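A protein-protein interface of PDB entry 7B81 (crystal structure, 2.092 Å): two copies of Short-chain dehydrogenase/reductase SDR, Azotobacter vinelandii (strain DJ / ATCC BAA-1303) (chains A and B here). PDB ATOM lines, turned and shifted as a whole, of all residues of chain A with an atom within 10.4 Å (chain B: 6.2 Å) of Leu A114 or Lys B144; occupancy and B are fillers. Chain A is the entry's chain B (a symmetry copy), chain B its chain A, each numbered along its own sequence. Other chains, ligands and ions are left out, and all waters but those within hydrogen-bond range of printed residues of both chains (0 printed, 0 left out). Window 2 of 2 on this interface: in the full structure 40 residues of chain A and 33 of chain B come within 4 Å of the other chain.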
ATOM      1  N   HIS A 111      16.743  -5.140 -18.807  1.00  0.00           N
ATOM      2  CA  HIS A 111      16.105  -5.373 -20.093  1.00  0.00           C
ATOM      3  C   HIS A 111      16.865  -6.464 -20.833  1.00  0.00           C
ATOM      4  O   HIS A 111      18.084  -6.594 -20.690  1.00  0.00           O
ATOM      5  CB  HIS A 111      16.060  -4.086 -20.925  1.00  0.00           C
ATOM      6  CG  HIS A 111      15.119  -4.149 -22.087  1.00  0.00           C
ATOM      7  ND1 HIS A 111      15.389  -4.877 -23.225  1.00  0.00           N
ATOM      8  CD2 HIS A 111      13.914  -3.565 -22.291  1.00  0.00           C
ATOM      9  CE1 HIS A 111      14.388  -4.746 -24.077  1.00  0.00           C
ATOM     10  NE2 HIS A 111      13.481  -3.954 -23.536  1.00  0.00           N
ATOM     11  N   SER A 112      16.131  -7.246 -21.620  1.00  0.00           N
ATOM     12  CA  SER A 112      16.756  -8.271 -22.441  1.00  0.00           C
ATOM     13  C   SER A 112      17.616  -7.631 -23.530  1.00  0.00           C
ATOM     14  O   SER A 112      17.478  -6.447 -23.853  1.00  0.00           O
ATOM     15  CB  SER A 112      15.701  -9.182 -23.065  1.00  0.00           C
ATOM     16  OG  SER A 112      16.314 -10.243 -23.777  1.00  0.00           O
ATOM     17  N   PHE A 113      18.508  -8.437 -24.107  1.00  0.00           N
ATOM     18  CA  PHE A 113      19.526  -7.910 -25.013  1.00  0.00           C
ATOM     19  C   PHE A 113      19.056  -7.835 -26.463  1.00  0.00           C
ATOM     20  O   PHE A 113      19.162  -6.777 -27.093  1.00  0.00           O
ATOM     21  CB  PHE A 113      20.798  -8.758 -24.932  1.00  0.00           C
ATOM     22  CG  PHE A 113      21.776  -8.481 -26.037  1.00  0.00           C
ATOM     23  CD1 PHE A 113      22.293  -7.208 -26.220  1.00  0.00           C
ATOM     24  CD2 PHE A 113      22.171  -9.488 -26.899  1.00  0.00           C
ATOM     25  CE1 PHE A 113      23.188  -6.945 -27.234  1.00  0.00           C
ATOM     26  CE2 PHE A 113      23.067  -9.232 -27.919  1.00  0.00           C
ATOM     27  CZ  PHE A 113      23.578  -7.958 -28.084  1.00  0.00           C
ATOM     28  N   LEU A 114      18.547  -8.944 -27.004  1.00  0.00           N
ATOM     29  CA  LEU A 114      18.236  -9.010 -28.430  1.00  0.00           C
ATOM     30  C   LEU A 114      17.110  -8.066 -28.835  1.00  0.00           C
ATOM     31  O   LEU A 114      16.981  -7.759 -30.026  1.00  0.00           O
ATOM     32  CB  LEU A 114      17.884 -10.444 -28.821  1.00  0.00           C
ATOM     33  CG  LEU A 114      18.989 -11.473 -28.587  1.00  0.00           C
ATOM     34  CD1 LEU A 114      18.455 -12.884 -28.730  1.00  0.00           C
ATOM     35  CD2 LEU A 114      20.143 -11.240 -29.542  1.00  0.00           C
ATOM     36  N   ASP A 115      16.304  -7.591 -27.883  1.00  0.00           N
ATOM     37  CA  ASP A 115      15.227  -6.647 -28.160  1.00  0.00           C
ATOM     38  C   ASP A 115      15.470  -5.303 -27.477  1.00  0.00           C
ATOM     39  O   ASP A 115      14.524  -4.599 -27.119  1.00  0.00           O
ATOM     40  CB  ASP A 115      13.877  -7.228 -27.743  1.00  0.00           C
ATOM     41  CG  ASP A 115      13.721  -7.325 -26.234  1.00  0.00           C
ATOM     42  OD1 ASP A 115      14.748  -7.487 -25.539  1.00  0.00           O
ATOM     43  OD2 ASP A 115      12.573  -7.238 -25.746  1.00  0.00           O
ATOM     44  N   MET A 116      16.731  -4.930 -27.302  1.00  0.00           N
ATOM     45  CA  MET A 116      17.050  -3.682 -26.621  1.00  0.00           C
ATOM     46  C   MET A 116      16.695  -2.493 -27.506  1.00  0.00           C
ATOM     47  O   MET A 116      17.105  -2.449 -28.673  1.00  0.00           O
ATOM     48  CB  MET A 116      18.532  -3.641 -26.250  1.00  0.00           C
ATOM     49  CG  MET A 116      18.984  -2.324 -25.640  1.00  0.00           C
ATOM     50  SD  MET A 116      18.434  -2.128 -23.936  1.00  0.00           S
ATOM     51  CE  MET A 116      18.971  -3.689 -23.243  1.00  0.00           C
ATOM     52  N   PRO A 117      15.935  -1.521 -27.003  1.00  0.00           N
ATOM     53  CA  PRO A 117      15.673  -0.312 -27.792  1.00  0.00           C
ATOM     54  C   PRO A 117      16.908   0.573 -27.864  1.00  0.00           C
ATOM     55  O   PRO A 117      17.665   0.698 -26.898  1.00  0.00           O
ATOM     56  CB  PRO A 117      14.536   0.381 -27.027  1.00  0.00           C
ATOM     57  CG  PRO A 117      14.013  -0.652 -26.061  1.00  0.00           C
ATOM     58  CD  PRO A 117      15.173  -1.534 -25.744  1.00  0.00           C
ATOM     59  N   ARG A 118      17.104   1.193 -29.031  1.00  0.00           N
ATOM     60  CA  ARG A 118      18.227   2.108 -29.200  1.00  0.00           C
ATOM     61  C   ARG A 118      18.159   3.267 -28.215  1.00  0.00           C
ATOM     62  O   ARG A 118      19.200   3.742 -27.746  1.00  0.00           O
ATOM     63  CB  ARG A 118      18.264   2.636 -30.632  1.00  0.00           C
ATOM     64  CG  ARG A 118      18.415   1.561 -31.693  1.00  0.00           C
ATOM     65  CD  ARG A 118      18.602   2.190 -33.060  1.00  0.00           C
ATOM     66  NE  ARG A 118      18.751   1.194 -34.116  1.00  0.00           N
ATOM     67  CZ  ARG A 118      19.143   1.478 -35.353  1.00  0.00           C
ATOM     68  NH1 ARG A 118      19.250   0.511 -36.256  1.00  0.00           N
ATOM     69  NH2 ARG A 118      19.430   2.729 -35.689  1.00  0.00           N
ATOM     70  N   LEU A 120      16.736   3.214 -25.139  1.00  0.00           N
ATOM     71  CA  LEU A 120      17.036   2.725 -23.798  1.00  0.00           C
ATOM     72  C   LEU A 120      18.534   2.540 -23.603  1.00  0.00           C
ATOM     73  O   LEU A 120      19.074   2.860 -22.535  1.00  0.00           O
ATOM     74  CB  LEU A 120      16.294   1.414 -23.542  1.00  0.00           C
ATOM     75  CG  LEU A 120      16.450   0.798 -22.153  1.00  0.00           C
ATOM     76  CD1 LEU A 120      15.938   1.754 -21.090  1.00  0.00           C
ATOM     77  CD2 LEU A 120      15.720  -0.533 -22.079  1.00  0.00           C
ATOM     78  N   GLY A 164      26.070  -9.837 -16.940  1.00  0.00           N
ATOM     79  CA  GLY A 164      24.685  -9.872 -16.512  1.00  0.00           C
ATOM     80  C   GLY A 164      23.768  -9.973 -17.711  1.00  0.00           C
ATOM     81  O   GLY A 164      23.800  -9.101 -18.586  1.00  0.00           O
ATOM     82  N   ALA A 165      22.953 -11.032 -17.765  1.00  0.00           N
ATOM     83  CA  ALA A 165      22.179 -11.312 -18.972  1.00  0.00           C
ATOM     84  C   ALA A 165      21.257 -10.154 -19.326  1.00  0.00           C
ATOM     85  O   ALA A 165      21.066  -9.840 -20.507  1.00  0.00           O
ATOM     86  CB  ALA A 165      21.375 -12.603 -18.796  1.00  0.00           C
ATOM     87  N   MET A 166      20.676  -9.506 -18.317  1.00  0.00           N
ATOM     88  CA  MET A 166      19.773  -8.380 -18.518  1.00  0.00           C
ATOM     89  C   MET A 166      20.476  -7.043 -18.326  1.00  0.00           C
ATOM     90  O   MET A 166      19.834  -6.044 -17.984  1.00  0.00           O
ATOM     91  CB  MET A 166      18.573  -8.495 -17.580  1.00  0.00           C
ATOM     92  CG  MET A 166      17.845  -9.822 -17.686  1.00  0.00           C
ATOM     93  SD  MET A 166      16.922  -9.956 -19.231  1.00  0.00           S
ATOM     94  CE  MET A 166      15.480  -8.973 -18.818  1.00  0.00           C
ATOM     95  N   GLN A 167      21.795  -7.006 -18.545  1.00  0.00           N
ATOM     96  CA  GLN A 167      22.584  -5.803 -18.324  1.00  0.00           C
ATOM     97  C   GLN A 167      23.637  -5.619 -19.413  1.00  0.00           C
ATOM     98  O   GLN A 167      24.716  -5.082 -19.147  1.00  0.00           O
ATOM     99  CB  GLN A 167      23.262  -5.834 -16.950  1.00  0.00           C
ATOM    100  CG  GLN A 167      22.313  -5.704 -15.769  1.00  0.00           C
ATOM    101  CD  GLN A 167      22.910  -6.244 -14.482  1.00  0.00           C
ATOM    102  OE1 GLN A 167      23.092  -7.453 -14.329  1.00  0.00           O
ATOM    103  NE2 GLN A 167      23.221  -5.349 -13.550  1.00  0.00           N
ATOM    104  N   THR A 168      23.344  -6.066 -20.638  1.00  0.00           N
ATOM    105  CA  THR A 168      24.294  -5.897 -21.733  1.00  0.00           C
ATOM    106  C   THR A 168      24.511  -4.427 -22.060  1.00  0.00           C
ATOM    107  O   THR A 168      25.572  -4.058 -22.573  1.00  0.00           O
ATOM    108  CB  THR A 168      23.817  -6.637 -22.980  1.00  0.00           C
ATOM    109  OG1 THR A 168      22.516  -6.161 -23.348  1.00  0.00           O
ATOM    110  CG2 THR A 168      23.770  -8.144 -22.733  1.00  0.00           C
ATOM    111  N   HIS A 169      23.524  -3.583 -21.785  1.00  0.00           N
ATOM    112  CA  HIS A 169      23.663  -2.143 -21.937  1.00  0.00           C
ATOM    113  C   HIS A 169      24.221  -1.471 -20.691  1.00  0.00           C
ATOM    114  O   HIS A 169      24.628  -0.305 -20.761  1.00  0.00           O
ATOM    115  CB  HIS A 169      22.306  -1.523 -22.282  1.00  0.00           C
ATOM    116  CG  HIS A 169      21.273  -1.704 -21.212  1.00  0.00           C
ATOM    117  ND1 HIS A 169      20.938  -2.941 -20.703  1.00  0.00           N
ATOM    118  CD2 HIS A 169      20.505  -0.805 -20.552  1.00  0.00           C
ATOM    119  CE1 HIS A 169      20.005  -2.796 -19.778  1.00  0.00           C
ATOM    120  NE2 HIS A 169      19.726  -1.510 -19.666  1.00  0.00           N
ATOM    121  N   TYR B 133      27.595  -2.677 -30.125  1.00  0.00           N
ATOM    122  CA  TYR B 133      26.476  -3.289 -29.414  1.00  0.00           C
ATOM    123  C   TYR B 133      25.404  -3.764 -30.387  1.00  0.00           C
ATOM    124  O   TYR B 133      25.017  -4.938 -30.384  1.00  0.00           O
ATOM    125  CB  TYR B 133      25.894  -2.288 -28.412  1.00  0.00           C
ATOM    126  CG  TYR B 133      24.767  -2.835 -27.561  1.00  0.00           C
ATOM    127  CD1 TYR B 133      25.031  -3.503 -26.374  1.00  0.00           C
ATOM    128  CD2 TYR B 133      23.440  -2.668 -27.937  1.00  0.00           C
ATOM    129  CE1 TYR B 133      24.006  -3.999 -25.588  1.00  0.00           C
ATOM    130  CE2 TYR B 133      22.410  -3.160 -27.158  1.00  0.00           C
ATOM    131  CZ  TYR B 133      22.699  -3.825 -25.985  1.00  0.00           C
ATOM    132  OH  TYR B 133      21.677  -4.316 -25.202  1.00  0.00           O
ATOM    133  N   VAL B 136      26.632  -6.457 -32.808  1.00  0.00           N
ATOM    134  CA  VAL B 136      26.543  -7.757 -32.153  1.00  0.00           C
ATOM    135  C   VAL B 136      25.087  -8.179 -32.017  1.00  0.00           C
ATOM    136  O   VAL B 136      24.745  -9.344 -32.247  1.00  0.00           O
ATOM    137  CB  VAL B 136      27.256  -7.725 -30.788  1.00  0.00           C
ATOM    138  CG1 VAL B 136      27.029  -9.032 -30.040  1.00  0.00           C
ATOM    139  CG2 VAL B 136      28.747  -7.473 -30.974  1.00  0.00           C
ATOM    140  N   GLN B 137      24.207  -7.240 -31.663  1.00  0.00           N
ATOM    141  CA  GLN B 137      22.793  -7.569 -31.490  1.00  0.00           C
ATOM    142  C   GLN B 137      22.182  -8.063 -32.793  1.00  0.00           C
ATOM    143  O   GLN B 137      21.491  -9.088 -32.818  1.00  0.00           O
ATOM    144  CB  GLN B 137      22.024  -6.353 -30.972  1.00  0.00           C
ATOM    145  CG  GLN B 137      20.538  -6.393 -31.306  1.00  0.00           C
ATOM    146  CD  GLN B 137      19.713  -5.475 -30.431  1.00  0.00           C
ATOM    147  OE1 GLN B 137      19.409  -4.343 -30.806  1.00  0.00           O
ATOM    148  NE2 GLN B 137      19.346  -5.961 -29.253  1.00  0.00           N
ATOM    149  N   ALA B 139      23.725  -9.308 -35.482  1.00  0.00           N
ATOM    150  CA  ALA B 139      24.311 -10.594 -35.851  1.00  0.00           C
ATOM    151  C   ALA B 139      23.787 -11.715 -34.962  1.00  0.00           C
ATOM    152  O   ALA B 139      23.561 -12.835 -35.433  1.00  0.00           O
ATOM    153  CB  ALA B 139      25.834 -10.520 -35.772  1.00  0.00           C
ATOM    154  N   ALA B 140      23.590 -11.432 -33.672  1.00  0.00           N
ATOM    155  CA  ALA B 140      23.121 -12.464 -32.754  1.00  0.00           C
ATOM    156  C   ALA B 140      21.692 -12.885 -33.074  1.00  0.00           C
ATOM    157  O   ALA B 140      21.352 -14.068 -32.970  1.00  0.00           O
ATOM    158  CB  ALA B 140      23.228 -11.973 -31.311  1.00  0.00           C
ATOM    159  N   ARG B 141      20.844 -11.930 -33.470  1.00  0.00           N
ATOM    160  CA  ARG B 141      19.461 -12.258 -33.802  1.00  0.00           C
ATOM    161  C   ARG B 141      19.393 -13.258 -34.948  1.00  0.00           C
ATOM    162  O   ARG B 141      18.530 -14.142 -34.959  1.00  0.00           O
ATOM    163  CB  ARG B 141      18.688 -10.983 -34.146  1.00  0.00           C
ATOM    164  N   ARG B 142      20.304 -13.142 -35.917  1.00  0.00           N
ATOM    165  CA  ARG B 142      20.349 -14.105 -37.014  1.00  0.00           C
ATOM    166  C   ARG B 142      20.828 -15.468 -36.528  1.00  0.00           C
ATOM    167  O   ARG B 142      20.301 -16.504 -36.954  1.00  0.00           O
ATOM    168  CB  ARG B 142      21.257 -13.582 -38.131  1.00  0.00           C
ATOM    169  CG  ARG B 142      21.649 -14.629 -39.166  1.00  0.00           C
ATOM    170  CD  ARG B 142      20.489 -14.960 -40.094  1.00  0.00           C
ATOM    171  NE  ARG B 142      20.664 -16.250 -40.759  1.00  0.00           N
ATOM    172  CZ  ARG B 142      19.857 -16.716 -41.708  1.00  0.00           C
ATOM    173  NH1 ARG B 142      20.091 -17.900 -42.260  1.00  0.00           N
ATOM    174  NH2 ARG B 142      18.816 -15.996 -42.108  1.00  0.00           N
ATOM    175  N   MET B 143      21.821 -15.485 -35.635  1.00  0.00           N
ATOM    176  CA  MET B 143      22.325 -16.752 -35.112  1.00  0.00           C
ATOM    177  C   MET B 143      21.258 -17.476 -34.303  1.00  0.00           C
ATOM    178  O   MET B 143      21.157 -18.707 -34.356  1.00  0.00           O
ATOM    179  CB  MET B 143      23.567 -16.512 -34.256  1.00  0.00           C
ATOM    180  CG  MET B 143      24.820 -16.188 -35.045  1.00  0.00           C
ATOM    181  SD  MET B 143      26.006 -15.285 -34.036  1.00  0.00           S
ATOM    182  CE  MET B 143      27.421 -15.222 -35.127  1.00  0.00           C
ATOM    183  N   LYS B 144      20.459 -16.729 -33.536  1.00  0.00           N
ATOM    184  CA  LYS B 144      19.372 -17.350 -32.786  1.00  0.00           C
ATOM    185  C   LYS B 144      18.285 -17.857 -33.723  1.00  0.00           C
ATOM    186  O   LYS B 144      17.796 -18.982 -33.562  1.00  0.00           O
ATOM    187  CB  LYS B 144      18.790 -16.360 -31.777  1.00  0.00           C
ATOM    188  CG  LYS B 144      17.564 -16.891 -31.036  1.00  0.00           C
ATOM    189  CD  LYS B 144      16.979 -15.848 -30.098  1.00  0.00           C
ATOM    190  CE  LYS B 144      15.660 -16.313 -29.499  1.00  0.00           C
ATOM    191  NZ  LYS B 144      14.965 -15.211 -28.774  1.00  0.00           N
ATOM    192  N   GLU B 145      17.904 -17.044 -34.713  1.00  0.00           N
ATOM    193  CA  GLU B 145      16.868 -17.442 -35.659  1.00  0.00           C
ATOM    194  C   GLU B 145      17.254 -18.700 -36.425  1.00  0.00           C
ATOM    195  O   GLU B 145      16.384 -19.512 -36.759  1.00  0.00           O
ATOM    196  CB  GLU B 145      16.576 -16.297 -36.630  1.00  0.00           C
ATOM    197  N   GLN B 146      18.546 -18.883 -36.712  1.00  0.00           N
ATOM    198  CA  GLN B 146      18.982 -20.115 -37.359  1.00  0.00           C
ATOM    199  C   GLN B 146      18.995 -21.284 -36.383  1.00  0.00           C
ATOM    200  O   GLN B 146      18.723 -22.424 -36.779  1.00  0.00           O
ATOM    201  CB  GLN B 146      20.368 -19.933 -37.979  1.00  0.00           C
ATOM    202  CG  GLN B 146      20.959 -21.226 -38.531  1.00  0.00           C
ATOM    203  CD  GLN B 146      22.318 -21.043 -39.175  1.00  0.00           C
ATOM    204  OE1 GLN B 146      22.955 -19.996 -39.039  1.00  0.00           O
ATOM    205  NE2 GLN B 146      22.773 -22.073 -39.884  1.00  0.00           N
ATOM    206  N   GLY B 147      19.300 -21.028 -35.116  1.00  0.00           N
ATOM    207  CA  GLY B 147      19.319 -22.094 -34.129  1.00  0.00           C
ATOM    208  C   GLY B 147      20.434 -23.097 -34.326  1.00  0.00           C
ATOM    209  O   GLY B 147      20.239 -24.293 -34.072  1.00  0.00           O
ATOM    210  N   ARG B 148      21.602 -22.641 -34.775  1.00  0.00           N
ATOM    211  CA  ARG B 148      22.753 -23.514 -34.968  1.00  0.00           C
ATOM    212  C   ARG B 148      23.974 -23.047 -34.186  1.00  0.00           C
ATOM    213  O   ARG B 148      25.089 -23.500 -34.468  1.00  0.00           O
ATOM    214  CB  ARG B 148      23.093 -23.623 -36.458  1.00  0.00           C
ATOM    215  N   GLY B 149      23.795 -22.161 -33.213  1.00  0.00           N
ATOM    216  CA  GLY B 149      24.918 -21.622 -32.481  1.00  0.00           C
ATOM    217  C   GLY B 149      25.631 -20.534 -33.261  1.00  0.00           C
ATOM    218  O   GLY B 149      25.146 -20.023 -34.276  1.00  0.00           O
ATOM    219  N   ALA B 187      23.680 -14.076 -21.928  1.00  0.00           N
ATOM    220  CA  ALA B 187      22.383 -14.033 -22.591  1.00  0.00           C
ATOM    221  C   ALA B 187      22.339 -14.935 -23.816  1.00  0.00           C
ATOM    222  O   ALA B 187      21.276 -15.468 -24.154  1.00  0.00           O
ATOM    223  CB  ALA B 187      22.039 -12.595 -22.979  1.00  0.00           C
ATOM    224  N   LEU B 188      23.473 -15.130 -24.483  1.00  0.00           N
ATOM    225  CA  LEU B 188      23.515 -15.909 -25.714  1.00  0.00           C
ATOM    226  C   LEU B 188      24.017 -17.334 -25.514  1.00  0.00           C
ATOM    227  O   LEU B 188      23.856 -18.159 -26.418  1.00  0.00           O
ATOM    228  CB  LEU B 188      24.386 -15.203 -26.755  1.00  0.00           C
ATOM    229  CG  LEU B 188      24.126 -13.711 -26.990  1.00  0.00           C
ATOM    230  CD1 LEU B 188      25.052 -13.136 -28.060  1.00  0.00           C
ATOM    231  CD2 LEU B 188      22.673 -13.454 -27.342  1.00  0.00           C
ATOM    232  N   TYR B 191      21.835 -20.354 -26.255  1.00  0.00           N
ATOM    233  CA  TYR B 191      21.527 -20.485 -27.672  1.00  0.00           C
ATOM    234  C   TYR B 191      22.730 -20.944 -28.493  1.00  0.00           C
ATOM    235  O   TYR B 191      22.715 -20.817 -29.724  1.00  0.00           O
ATOM    236  CB  TYR B 191      20.996 -19.158 -28.223  1.00  0.00           C
ATOM    237  CG  TYR B 191      19.895 -18.517 -27.407  1.00  0.00           C
ATOM    238  CD1 TYR B 191      19.040 -19.282 -26.620  1.00  0.00           C
ATOM    239  CD2 TYR B 191      19.706 -17.141 -27.428  1.00  0.00           C
ATOM    240  CE1 TYR B 191      18.037 -18.692 -25.875  1.00  0.00           C
ATOM    241  CE2 TYR B 191      18.702 -16.545 -26.686  1.00  0.00           C
ATOM    242  CZ  TYR B 191      17.871 -17.326 -25.911  1.00  0.00           C
ATOM    243  OH  TYR B 191      16.868 -16.746 -25.167  1.00  0.00           O
ATOM    244  N   ILE B 193      25.629 -19.590 -28.705  1.00  0.00           N
ATOM    245  CA  ILE B 193      26.393 -18.456 -29.209  1.00  0.00           C
ATOM    246  C   ILE B 193      27.479 -18.126 -28.194  1.00  0.00           C
ATOM    247  O   ILE B 193      27.188 -17.654 -27.088  1.00  0.00           O
ATOM    248  CB  ILE B 193      25.491 -17.243 -29.470  1.00  0.00           C
ATOM    249  CG1 ILE B 193      24.218 -17.672 -30.203  1.00  0.00           C
ATOM    250  CG2 ILE B 193      26.241 -16.175 -30.249  1.00  0.00           C
ATOM    251  CD1 ILE B 193      23.218 -16.552 -30.382  1.00  0.00           C
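The side-chain hydroxyl (OH) of Tyr B133 sits at hydrogen-bond distance from the side-chain hydroxyl (OG1) of Thr A168.
O of Phe A113 sits close to NE2 of Gln B137, 2.3 Å away.
The side-chain amide nitrogen (NE2) of Gln B137 sits close to the backbone NH (N) of Met A116 (3.4 Å).
NE2 of Gln B137 lies within hydrogen-bond range of O of Leu A114 (3.1 Å).
Phe A113 touches Tyr B133.
Leu A114 touches Ala B140 (CD2 to CB, 3.6 Å).
Leu A114 touches Lys B144 (CD1 to CD, 3.6 Å).
Gln B137 touches Asp A115.
Tyr B133 touches Met A116 (OH to CG, 3.4 Å).
Ala A165 touches Ala B187.
His A169 touches Tyr B133 (N to CE1, 3.9 Å).
Printed residues of chain B within 4 Å of Phe A113: Tyr B133 and Gln B137.
Printed residues of chain B within 4 Å of Leu A114: Gln B137 (3.1 Å), Ala B140 (3.6 Å) and Lys B144 (3.6 Å).
Of the printed residues of chain B, Asp A115 touches Gln B137 (3.7 Å).
Of the printed residues of chain B, Ala A165 touches Ala B187 (3.8 Å).
Gln B137 touches just these residues of chain A: Phe A113, Leu A114, Asp A115 and Met A116.
No residue of chain A comes within 4 Å of Arg B141.
Of the printed residues of chain A, Lys B144 touches Leu A114 (3.6 Å).
No residue of chain A comes within 4 Å of Glu B145.
No residue of chain A comes within 4 Å of Gly B147.
Of the printed residues of chain A, Ala B187 touches Ala A165 (3.8 Å).
The nearest printed residue of chain B that does not touch Leu A114 is Leu B188 (4.02 Å).
The nearest printed residue of chain A that does not touch Tyr B133 is Ser A112 (4.9 Å).
Hydrophobic or aromatic side chains of chain B within 4 Å of the printed part of chain A: Tyr B133, Ala B140 and Ala B187.
Of the 15 printed residues of chain A, 7 touch a printed residue of chain B.
Among the printed residues, 11 pairs touch across the chains.
No position is printed for both chains.
Of the 11 pairs that touch across the chains among the printed residues, none has its exchanged pair printed and touching as well.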
